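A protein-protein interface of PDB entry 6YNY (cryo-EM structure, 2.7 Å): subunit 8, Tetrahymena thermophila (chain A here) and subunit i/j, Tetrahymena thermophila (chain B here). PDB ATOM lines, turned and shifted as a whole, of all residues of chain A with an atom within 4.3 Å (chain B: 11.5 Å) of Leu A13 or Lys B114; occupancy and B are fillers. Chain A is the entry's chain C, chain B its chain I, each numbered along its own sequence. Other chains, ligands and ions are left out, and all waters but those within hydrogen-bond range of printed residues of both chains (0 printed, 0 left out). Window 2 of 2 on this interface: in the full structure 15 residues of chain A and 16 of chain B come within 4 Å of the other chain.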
ATOM      1  N   LEU A  11     -32.545 -32.492 -16.273  1.00  0.00           N
ATOM      2  CA  LEU A  11     -32.115 -31.146 -16.613  1.00  0.00           C
ATOM      3  C   LEU A  11     -31.345 -30.472 -15.489  1.00  0.00           C
ATOM      4  O   LEU A  11     -30.859 -29.352 -15.677  1.00  0.00           O
ATOM      5  CB  LEU A  11     -33.328 -30.292 -16.977  1.00  0.00           C
ATOM      6  CG  LEU A  11     -34.222 -30.829 -18.086  1.00  0.00           C
ATOM      7  CD1 LEU A  11     -35.418 -29.930 -18.259  1.00  0.00           C
ATOM      8  CD2 LEU A  11     -33.451 -30.955 -19.377  1.00  0.00           C
ATOM      9  N   ASP A  12     -31.224 -31.120 -14.336  1.00  0.00           N
ATOM     10  CA  ASP A  12     -30.596 -30.510 -13.177  1.00  0.00           C
ATOM     11  C   ASP A  12     -29.084 -30.655 -13.234  1.00  0.00           C
ATOM     12  O   ASP A  12     -28.561 -31.741 -13.505  1.00  0.00           O
ATOM     13  CB  ASP A  12     -31.132 -31.144 -11.898  1.00  0.00           C
ATOM     14  CG  ASP A  12     -30.565 -30.506 -10.650  1.00  0.00           C
ATOM     15  OD1 ASP A  12     -30.873 -29.325 -10.392  1.00  0.00           O
ATOM     16  OD2 ASP A  12     -29.814 -31.186  -9.923  1.00  0.00           O
ATOM     17  N   LEU A  13     -28.386 -29.551 -12.979  1.00  0.00           N
ATOM     18  CA  LEU A  13     -26.947 -29.561 -12.789  1.00  0.00           C
ATOM     19  C   LEU A  13     -26.515 -28.905 -11.491  1.00  0.00           C
ATOM     20  O   LEU A  13     -25.327 -28.966 -11.158  1.00  0.00           O
ATOM     21  CB  LEU A  13     -26.236 -28.868 -13.959  1.00  0.00           C
ATOM     22  CG  LEU A  13     -26.388 -29.551 -15.317  1.00  0.00           C
ATOM     23  CD1 LEU A  13     -25.736 -28.726 -16.390  1.00  0.00           C
ATOM     24  CD2 LEU A  13     -25.792 -30.949 -15.299  1.00  0.00           C
ATOM     25  N   ASN A  14     -27.432 -28.285 -10.746  1.00  0.00           N
ATOM     26  CA  ASN A  14     -27.073 -27.710  -9.457  1.00  0.00           C
ATOM     27  C   ASN A  14     -26.715 -28.795  -8.454  1.00  0.00           C
ATOM     28  O   ASN A  14     -25.804 -28.621  -7.637  1.00  0.00           O
ATOM     29  CB  ASN A  14     -28.225 -26.870  -8.915  1.00  0.00           C
ATOM     30  CG  ASN A  14     -28.538 -25.677  -9.775  1.00  0.00           C
ATOM     31  OD1 ASN A  14     -27.678 -25.152 -10.479  1.00  0.00           O
ATOM     32  ND2 ASN A  14     -29.783 -25.235  -9.718  1.00  0.00           N
ATOM     33  N   ASP A  15     -27.424 -29.921  -8.501  1.00  0.00           N
ATOM     34  CA  ASP A  15     -27.262 -30.998  -7.536  1.00  0.00           C
ATOM     35  C   ASP A  15     -26.806 -32.291  -8.195  1.00  0.00           C
ATOM     36  O   ASP A  15     -27.026 -33.374  -7.648  1.00  0.00           O
ATOM     37  CB  ASP A  15     -28.570 -31.218  -6.779  1.00  0.00           C
ATOM     38  CG  ASP A  15     -29.030 -29.978  -6.043  1.00  0.00           C
ATOM     39  OD1 ASP A  15     -28.189 -29.329  -5.387  1.00  0.00           O
ATOM     40  OD2 ASP A  15     -30.230 -29.646  -6.131  1.00  0.00           O
ATOM     41  N   ASP A  16     -26.172 -32.202  -9.364  1.00  0.00           N
ATOM     42  CA  ASP A  16     -25.667 -33.399 -10.019  1.00  0.00           C
ATOM     43  C   ASP A  16     -24.578 -34.075  -9.202  1.00  0.00           C
ATOM     44  O   ASP A  16     -24.336 -35.272  -9.385  1.00  0.00           O
ATOM     45  CB  ASP A  16     -25.139 -33.059 -11.411  1.00  0.00           C
ATOM     46  CG  ASP A  16     -24.802 -34.292 -12.220  1.00  0.00           C
ATOM     47  OD1 ASP A  16     -25.255 -35.391 -11.844  1.00  0.00           O
ATOM     48  OD2 ASP A  16     -24.081 -34.165 -13.230  1.00  0.00           O
ATOM     49  N   PHE A  23     -21.497 -35.895 -15.853  1.00  0.00           N
ATOM     50  CA  PHE A  23     -21.805 -35.081 -17.022  1.00  0.00           C
ATOM     51  C   PHE A  23     -20.800 -33.951 -17.191  1.00  0.00           C
ATOM     52  O   PHE A  23     -20.350 -33.670 -18.308  1.00  0.00           O
ATOM     53  CB  PHE A  23     -23.222 -34.525 -16.898  1.00  0.00           C
ATOM     54  CG  PHE A  23     -23.637 -33.651 -18.039  1.00  0.00           C
ATOM     55  CD1 PHE A  23     -24.239 -34.192 -19.156  1.00  0.00           C
ATOM     56  CD2 PHE A  23     -23.437 -32.285 -17.990  1.00  0.00           C
ATOM     57  CE1 PHE A  23     -24.625 -33.390 -20.201  1.00  0.00           C
ATOM     58  CE2 PHE A  23     -23.820 -31.483 -19.033  1.00  0.00           C
ATOM     59  CZ  PHE A  23     -24.415 -32.035 -20.141  1.00  0.00           C
ATOM     60  N   GLU A  24     -20.424 -33.298 -16.092  1.00  0.00           N
ATOM     61  CA  GLU A  24     -19.537 -32.144 -16.168  1.00  0.00           C
ATOM     62  C   GLU A  24     -18.178 -32.478 -16.767  1.00  0.00           C
ATOM     63  O   GLU A  24     -17.474 -31.564 -17.209  1.00  0.00           O
ATOM     64  CB  GLU A  24     -19.364 -31.533 -14.776  1.00  0.00           C
ATOM     65  CG  GLU A  24     -18.927 -32.507 -13.704  1.00  0.00           C
ATOM     66  CD  GLU A  24     -18.814 -31.860 -12.340  1.00  0.00           C
ATOM     67  OE1 GLU A  24     -19.197 -30.680 -12.211  1.00  0.00           O
ATOM     68  OE2 GLU A  24     -18.344 -32.529 -11.397  1.00  0.00           O
ATOM     69  N   ILE A  27     -18.688 -34.193 -21.275  1.00  0.00           N
ATOM     70  CA  ILE A  27     -18.929 -33.270 -22.378  1.00  0.00           C
ATOM     71  C   ILE A  27     -17.647 -32.565 -22.788  1.00  0.00           C
ATOM     72  O   ILE A  27     -17.516 -32.120 -23.934  1.00  0.00           O
ATOM     73  CB  ILE A  27     -20.030 -32.261 -22.008  1.00  0.00           C
ATOM     74  CG1 ILE A  27     -19.634 -31.463 -20.773  1.00  0.00           C
ATOM     75  CG2 ILE A  27     -21.335 -32.974 -21.777  1.00  0.00           C
ATOM     76  CD1 ILE A  27     -20.602 -30.384 -20.438  1.00  0.00           C
ATOM     77  N   ILE A  28     -16.685 -32.441 -21.873  1.00  0.00           N
ATOM     78  CA  ILE A  28     -15.386 -31.891 -22.240  1.00  0.00           C
ATOM     79  C   ILE A  28     -14.762 -32.723 -23.350  1.00  0.00           C
ATOM     80  O   ILE A  28     -14.266 -32.192 -24.348  1.00  0.00           O
ATOM     81  CB  ILE A  28     -14.469 -31.819 -21.007  1.00  0.00           C
ATOM     82  CG1 ILE A  28     -14.995 -30.779 -20.024  1.00  0.00           C
ATOM     83  CG2 ILE A  28     -13.046 -31.500 -21.423  1.00  0.00           C
ATOM     84  CD1 ILE A  28     -14.287 -30.788 -18.698  1.00  0.00           C
ATOM     85  N   ALA B 101     -23.832 -32.184 -30.253  1.00  0.00           N
ATOM     86  CA  ALA B 101     -23.280 -31.851 -28.949  1.00  0.00           C
ATOM     87  C   ALA B 101     -22.471 -30.566 -28.992  1.00  0.00           C
ATOM     88  O   ALA B 101     -22.290 -29.927 -27.953  1.00  0.00           O
ATOM     89  CB  ALA B 101     -22.415 -33.001 -28.437  1.00  0.00           C
ATOM     90  N   GLY B 102     -21.989 -30.175 -30.170  1.00  0.00           N
ATOM     91  CA  GLY B 102     -21.250 -28.941 -30.320  1.00  0.00           C
ATOM     92  C   GLY B 102     -22.077 -27.694 -30.115  1.00  0.00           C
ATOM     93  O   GLY B 102     -21.501 -26.612 -29.960  1.00  0.00           O
ATOM     94  N   LEU B 103     -23.404 -27.815 -30.112  1.00  0.00           N
ATOM     95  CA  LEU B 103     -24.254 -26.667 -29.834  1.00  0.00           C
ATOM     96  C   LEU B 103     -24.132 -26.208 -28.391  1.00  0.00           C
ATOM     97  O   LEU B 103     -24.464 -25.059 -28.089  1.00  0.00           O
ATOM     98  CB  LEU B 103     -25.705 -27.003 -30.161  1.00  0.00           C
ATOM     99  CG  LEU B 103     -25.964 -27.339 -31.627  1.00  0.00           C
ATOM    100  CD1 LEU B 103     -27.341 -27.911 -31.809  1.00  0.00           C
ATOM    101  CD2 LEU B 103     -25.795 -26.110 -32.493  1.00  0.00           C
ATOM    102  N   GLY B 104     -23.668 -27.075 -27.498  1.00  0.00           N
ATOM    103  CA  GLY B 104     -23.424 -26.719 -26.120  1.00  0.00           C
ATOM    104  C   GLY B 104     -21.983 -26.360 -25.844  1.00  0.00           C
ATOM    105  O   GLY B 104     -21.590 -26.284 -24.675  1.00  0.00           O
ATOM    106  N   LEU B 105     -21.187 -26.127 -26.888  1.00  0.00           N
ATOM    107  CA  LEU B 105     -19.782 -25.785 -26.707  1.00  0.00           C
ATOM    108  C   LEU B 105     -19.627 -24.526 -25.870  1.00  0.00           C
ATOM    109  O   LEU B 105     -18.832 -24.486 -24.925  1.00  0.00           O
ATOM    110  CB  LEU B 105     -19.121 -25.615 -28.071  1.00  0.00           C
ATOM    111  CG  LEU B 105     -17.649 -25.208 -28.091  1.00  0.00           C
ATOM    112  CD1 LEU B 105     -16.797 -26.294 -27.498  1.00  0.00           C
ATOM    113  CD2 LEU B 105     -17.212 -24.908 -29.500  1.00  0.00           C
ATOM    114  N   PHE B 106     -20.386 -23.485 -26.201  1.00  0.00           N
ATOM    115  CA  PHE B 106     -20.281 -22.216 -25.498  1.00  0.00           C
ATOM    116  C   PHE B 106     -21.263 -22.100 -24.345  1.00  0.00           C
ATOM    117  O   PHE B 106     -20.967 -21.416 -23.361  1.00  0.00           O
ATOM    118  CB  PHE B 106     -20.503 -21.062 -26.473  1.00  0.00           C
ATOM    119  CG  PHE B 106     -19.719 -21.187 -27.739  1.00  0.00           C
ATOM    120  CD1 PHE B 106     -18.348 -21.057 -27.731  1.00  0.00           C
ATOM    121  CD2 PHE B 106     -20.353 -21.432 -28.941  1.00  0.00           C
ATOM    122  CE1 PHE B 106     -17.627 -21.173 -28.887  1.00  0.00           C
ATOM    123  CE2 PHE B 106     -19.633 -21.544 -30.100  1.00  0.00           C
ATOM    124  CZ  PHE B 106     -18.268 -21.415 -30.073  1.00  0.00           C
ATOM    125  N   VAL B 107     -22.422 -22.749 -24.439  1.00  0.00           N
ATOM    126  CA  VAL B 107     -23.355 -22.740 -23.319  1.00  0.00           C
ATOM    127  C   VAL B 107     -22.699 -23.341 -22.088  1.00  0.00           C
ATOM    128  O   VAL B 107     -22.834 -22.821 -20.975  1.00  0.00           O
ATOM    129  CB  VAL B 107     -24.646 -23.490 -23.688  1.00  0.00           C
ATOM    130  CG1 VAL B 107     -25.542 -23.607 -22.486  1.00  0.00           C
ATOM    131  CG2 VAL B 107     -25.358 -22.781 -24.807  1.00  0.00           C
ATOM    132  N   TYR B 108     -21.976 -24.441 -22.267  1.00  0.00           N
ATOM    133  CA  TYR B 108     -21.240 -25.081 -21.188  1.00  0.00           C
ATOM    134  C   TYR B 108     -19.758 -24.911 -21.494  1.00  0.00           C
ATOM    135  O   TYR B 108     -19.097 -25.806 -22.017  1.00  0.00           O
ATOM    136  CB  TYR B 108     -21.635 -26.538 -21.060  1.00  0.00           C
ATOM    137  CG  TYR B 108     -23.124 -26.747 -21.044  1.00  0.00           C
ATOM    138  CD1 TYR B 108     -23.847 -26.604 -19.877  1.00  0.00           C
ATOM    139  CD2 TYR B 108     -23.808 -27.078 -22.199  1.00  0.00           C
ATOM    140  CE1 TYR B 108     -25.205 -26.784 -19.857  1.00  0.00           C
ATOM    141  CE2 TYR B 108     -25.167 -27.262 -22.189  1.00  0.00           C
ATOM    142  CZ  TYR B 108     -25.860 -27.115 -21.015  1.00  0.00           C
ATOM    143  OH  TYR B 108     -27.219 -27.295 -21.000  1.00  0.00           O
ATOM    144  N   TRP B 109     -19.233 -23.745 -21.137  1.00  0.00           N
ATOM    145  CA  TRP B 109     -17.818 -23.432 -21.257  1.00  0.00           C
ATOM    146  C   TRP B 109     -17.324 -23.051 -19.875  1.00  0.00           C
ATOM    147  O   TRP B 109     -17.841 -22.111 -19.263  1.00  0.00           O
ATOM    148  CB  TRP B 109     -17.563 -22.300 -22.250  1.00  0.00           C
ATOM    149  CG  TRP B 109     -16.108 -22.059 -22.485  1.00  0.00           C
ATOM    150  CD1 TRP B 109     -15.217 -21.526 -21.605  1.00  0.00           C
ATOM    151  CD2 TRP B 109     -15.371 -22.339 -23.679  1.00  0.00           C
ATOM    152  NE1 TRP B 109     -13.975 -21.461 -22.170  1.00  0.00           N
ATOM    153  CE2 TRP B 109     -14.041 -21.951 -23.444  1.00  0.00           C
ATOM    154  CE3 TRP B 109     -15.705 -22.878 -24.922  1.00  0.00           C
ATOM    155  CZ2 TRP B 109     -13.048 -22.086 -24.403  1.00  0.00           C
ATOM    156  CZ3 TRP B 109     -14.717 -23.011 -25.871  1.00  0.00           C
ATOM    157  CH2 TRP B 109     -13.405 -22.616 -25.607  1.00  0.00           C
ATOM    158  N   GLY B 110     -16.330 -23.775 -19.391  1.00  0.00           N
ATOM    159  CA  GLY B 110     -15.821 -23.567 -18.059  1.00  0.00           C
ATOM    160  C   GLY B 110     -16.612 -24.328 -17.018  1.00  0.00           C
ATOM    161  O   GLY B 110     -17.700 -24.853 -17.260  1.00  0.00           O
ATOM    162  N   ASP B 111     -16.041 -24.368 -15.818  1.00  0.00           N
ATOM    163  CA  ASP B 111     -16.628 -25.148 -14.739  1.00  0.00           C
ATOM    164  C   ASP B 111     -17.895 -24.497 -14.198  1.00  0.00           C
ATOM    165  O   ASP B 111     -18.848 -25.194 -13.830  1.00  0.00           O
ATOM    166  CB  ASP B 111     -15.598 -25.320 -13.630  1.00  0.00           C
ATOM    167  CG  ASP B 111     -14.307 -25.940 -14.129  1.00  0.00           C
ATOM    168  OD1 ASP B 111     -14.375 -26.868 -14.961  1.00  0.00           O
ATOM    169  OD2 ASP B 111     -13.224 -25.493 -13.697  1.00  0.00           O
ATOM    170  N   ASP B 112     -17.930 -23.165 -14.156  1.00  0.00           N
ATOM    171  CA  ASP B 112     -19.066 -22.469 -13.562  1.00  0.00           C
ATOM    172  C   ASP B 112     -20.362 -22.728 -14.315  1.00  0.00           C
ATOM    173  O   ASP B 112     -21.443 -22.676 -13.718  1.00  0.00           O
ATOM    174  CB  ASP B 112     -18.785 -20.971 -13.511  1.00  0.00           C
ATOM    175  CG  ASP B 112     -17.509 -20.641 -12.769  1.00  0.00           C
ATOM    176  OD1 ASP B 112     -16.865 -21.574 -12.248  1.00  0.00           O
ATOM    177  OD2 ASP B 112     -17.147 -19.447 -12.713  1.00  0.00           O
ATOM    178  N   ASN B 113     -20.287 -23.001 -15.611  1.00  0.00           N
ATOM    179  CA  ASN B 113     -21.479 -23.201 -16.422  1.00  0.00           C
ATOM    180  C   ASN B 113     -21.944 -24.648 -16.462  1.00  0.00           C
ATOM    181  O   ASN B 113     -22.949 -24.940 -17.116  1.00  0.00           O
ATOM    182  CB  ASN B 113     -21.233 -22.709 -17.846  1.00  0.00           C
ATOM    183  CG  ASN B 113     -21.125 -21.209 -17.932  1.00  0.00           C
ATOM    184  OD1 ASN B 113     -21.836 -20.482 -17.242  1.00  0.00           O
ATOM    185  ND2 ASN B 113     -20.232 -20.736 -18.781  1.00  0.00           N
ATOM    186  N   LYS B 114     -21.248 -25.557 -15.786  1.00  0.00           N
ATOM    187  CA  LYS B 114     -21.630 -26.959 -15.750  1.00  0.00           C
ATOM    188  C   LYS B 114     -22.225 -27.375 -14.415  1.00  0.00           C
ATOM    189  O   LYS B 114     -22.647 -28.526 -14.276  1.00  0.00           O
ATOM    190  CB  LYS B 114     -20.421 -27.844 -16.055  1.00  0.00           C
ATOM    191  CG  LYS B 114     -19.706 -27.518 -17.344  1.00  0.00           C
ATOM    192  CD  LYS B 114     -18.537 -28.450 -17.557  1.00  0.00           C
ATOM    193  CE  LYS B 114     -17.497 -27.869 -18.487  1.00  0.00           C
ATOM    194  NZ  LYS B 114     -18.029 -27.533 -19.808  1.00  0.00           N
ATOM    195  N   CYS B 115     -22.272 -26.482 -13.434  1.00  0.00           N
ATOM    196  CA  CYS B 115     -22.754 -26.834 -12.107  1.00  0.00           C
ATOM    197  C   CYS B 115     -23.120 -25.560 -11.359  1.00  0.00           C
ATOM    198  O   CYS B 115     -23.084 -24.457 -11.915  1.00  0.00           O
ATOM    199  CB  CYS B 115     -21.699 -27.635 -11.340  1.00  0.00           C
ATOM    200  SG  CYS B 115     -20.300 -26.658 -10.752  1.00  0.00           S
ATOM    201  N   TYR B 116     -23.479 -25.724 -10.090  1.00  0.00           N
ATOM    202  CA  TYR B 116     -23.769 -24.614  -9.189  1.00  0.00           C
ATOM    203  C   TYR B 116     -22.457 -24.210  -8.531  1.00  0.00           C
ATOM    204  O   TYR B 116     -22.008 -24.839  -7.572  1.00  0.00           O
ATOM    205  CB  TYR B 116     -24.826 -25.025  -8.174  1.00  0.00           C
ATOM    206  CG  TYR B 116     -25.240 -23.942  -7.218  1.00  0.00           C
ATOM    207  CD1 TYR B 116     -25.910 -22.818  -7.663  1.00  0.00           C
ATOM    208  CD2 TYR B 116     -24.984 -24.056  -5.866  1.00  0.00           C
ATOM    209  CE1 TYR B 116     -26.295 -21.830  -6.788  1.00  0.00           C
ATOM    210  CE2 TYR B 116     -25.365 -23.080  -4.987  1.00  0.00           C
ATOM    211  CZ  TYR B 116     -26.021 -21.970  -5.449  1.00  0.00           C
ATOM    212  OH  TYR B 116     -26.397 -21.000  -4.559  1.00  0.00           O
ATOM    213  N   SER B 117     -21.837 -23.159  -9.062  1.00  0.00           N
ATOM    214  CA  SER B 117     -20.491 -22.804  -8.638  1.00  0.00           C
ATOM    215  C   SER B 117     -20.373 -22.468  -7.154  1.00  0.00           C
ATOM    216  O   SER B 117     -19.320 -22.781  -6.573  1.00  0.00           O
ATOM    217  CB  SER B 117     -19.988 -21.637  -9.500  1.00  0.00           C
ATOM    218  OG  SER B 117     -20.820 -20.501  -9.377  1.00  0.00           O
ATOM    219  N   PRO B 118     -21.356 -21.851  -6.496  1.00  0.00           N
ATOM    220  CA  PRO B 118     -21.191 -21.543  -5.067  1.00  0.00           C
ATOM    221  C   PRO B 118     -20.951 -22.758  -4.195  1.00  0.00           C
ATOM    222  O   PRO B 118     -20.498 -22.599  -3.055  1.00  0.00           O
ATOM    223  CB  PRO B 118     -22.505 -20.841  -4.709  1.00  0.00           C
ATOM    224  CG  PRO B 118     -22.995 -20.304  -5.982  1.00  0.00           C
ATOM    225  CD  PRO B 118     -22.616 -21.300  -7.015  1.00  0.00           C
ATOM    226  N   ASP B 119     -21.239 -23.961  -4.680  1.00  0.00           N
ATOM    227  CA  ASP B 119     -20.926 -25.185  -3.960  1.00  0.00           C
ATOM    228  C   ASP B 119     -19.556 -25.739  -4.317  1.00  0.00           C
ATOM    229  O   ASP B 119     -19.213 -26.840  -3.880  1.00  0.00           O
ATOM    230  CB  ASP B 119     -21.992 -26.243  -4.233  1.00  0.00           C
ATOM    231  CG  ASP B 119     -23.294 -25.959  -3.517  1.00  0.00           C
ATOM    232  OD1 ASP B 119     -23.376 -24.934  -2.811  1.00  0.00           O
ATOM    233  OD2 ASP B 119     -24.235 -26.767  -3.656  1.00  0.00           O
ATOM    234  N   ARG B 120     -18.772 -25.004  -5.096  1.00  0.00           N
ATOM    235  CA  ARG B 120     -17.440 -25.420  -5.495  1.00  0.00           C
ATOM    236  C   ARG B 120     -16.377 -24.510  -4.893  1.00  0.00           C
ATOM    237  O   ARG B 120     -16.618 -23.334  -4.613  1.00  0.00           O
ATOM    238  CB  ARG B 120     -17.302 -25.429  -7.018  1.00  0.00           C
ATOM    239  CG  ARG B 120     -18.241 -26.373  -7.727  1.00  0.00           C
ATOM    240  CD  ARG B 120     -18.105 -27.765  -7.190  1.00  0.00           C
ATOM    241  NE  ARG B 120     -18.527 -28.784  -8.142  1.00  0.00           N
ATOM    242  CZ  ARG B 120     -19.789 -29.087  -8.401  1.00  0.00           C
ATOM    243  NH1 ARG B 120     -20.772 -28.442  -7.795  1.00  0.00           N
ATOM    244  NH2 ARG B 120     -20.060 -30.037  -9.276  1.00  0.00           N
ATOM    245  N   PRO B 122     -13.511 -23.140  -6.125  1.00  0.00           N
ATOM    246  CA  PRO B 122     -13.023 -21.937  -6.819  1.00  0.00           C
ATOM    247  C   PRO B 122     -13.871 -20.704  -6.592  1.00  0.00           C
ATOM    248  O   PRO B 122     -13.361 -19.588  -6.746  1.00  0.00           O
ATOM    249  CB  PRO B 122     -13.038 -22.358  -8.293  1.00  0.00           C
ATOM    250  CG  PRO B 122     -12.984 -23.820  -8.268  1.00  0.00           C
ATOM    251  CD  PRO B 122     -13.741 -24.242  -7.067  1.00  0.00           C
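The guanidinium group (NH2) of Arg B120 is in salt-bridge range of the side-chain carboxylate (OE1) of Glu A24, 3.1 Å away.
The side-chain sulfur (SG) of Cys B115 lies close to the guanidinium group (NH1) of Arg B120, 3.5 Å away. NZ of Lys B114 is in hydrogen-bond range of O of Tyr B108. O of Asp B111 lies within hydrogen-bond range of SG of Cys B115, at 3.7 Å.
Among the printed residues, merely in contact across the chains: Glu A24 with Lys B114, Leu A13 with Cys B115, Leu A13 with Lys B114, Asn A14 with Tyr B116, Leu A13 with Tyr B116 and Ile A27 with Lys B114.
Printed residues of chain B within 4 Å of Leu A13: Lys B114 (3.6 Å), Cys B115 (3.5 Å) and Tyr B116 (3.9 Å). No residue of chain B comes within 4 Å of Asp A16. No residue of chain B comes within 4 Å of Phe A23. Of chain B, only Lys B114 and Arg B120 come within 4 Å of Glu A24. Phe B106 touches none of the printed residues of chain A. Lys B114 touches just these residues of chain A: Leu A13 (3.6 Å), Glu A24 (3.3 Å) and Ile A27 (3.9 Å). Of the printed residues of chain A, Tyr B116 touches Leu A13 and Asn A14. Of the printed residues of chain A, Arg B120 touches Glu A24 (3.1 Å). The nearest printed residue of chain B that does not touch Leu A13 is Tyr B108 (4.01 Å).
Of the 21 printed residues of chain B, 4 touch a printed residue of chain A. Of the 10 printed residues of chain A, 4 touch a printed residue of chain B. Among the printed residues, 7 pairs touch across the chains.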
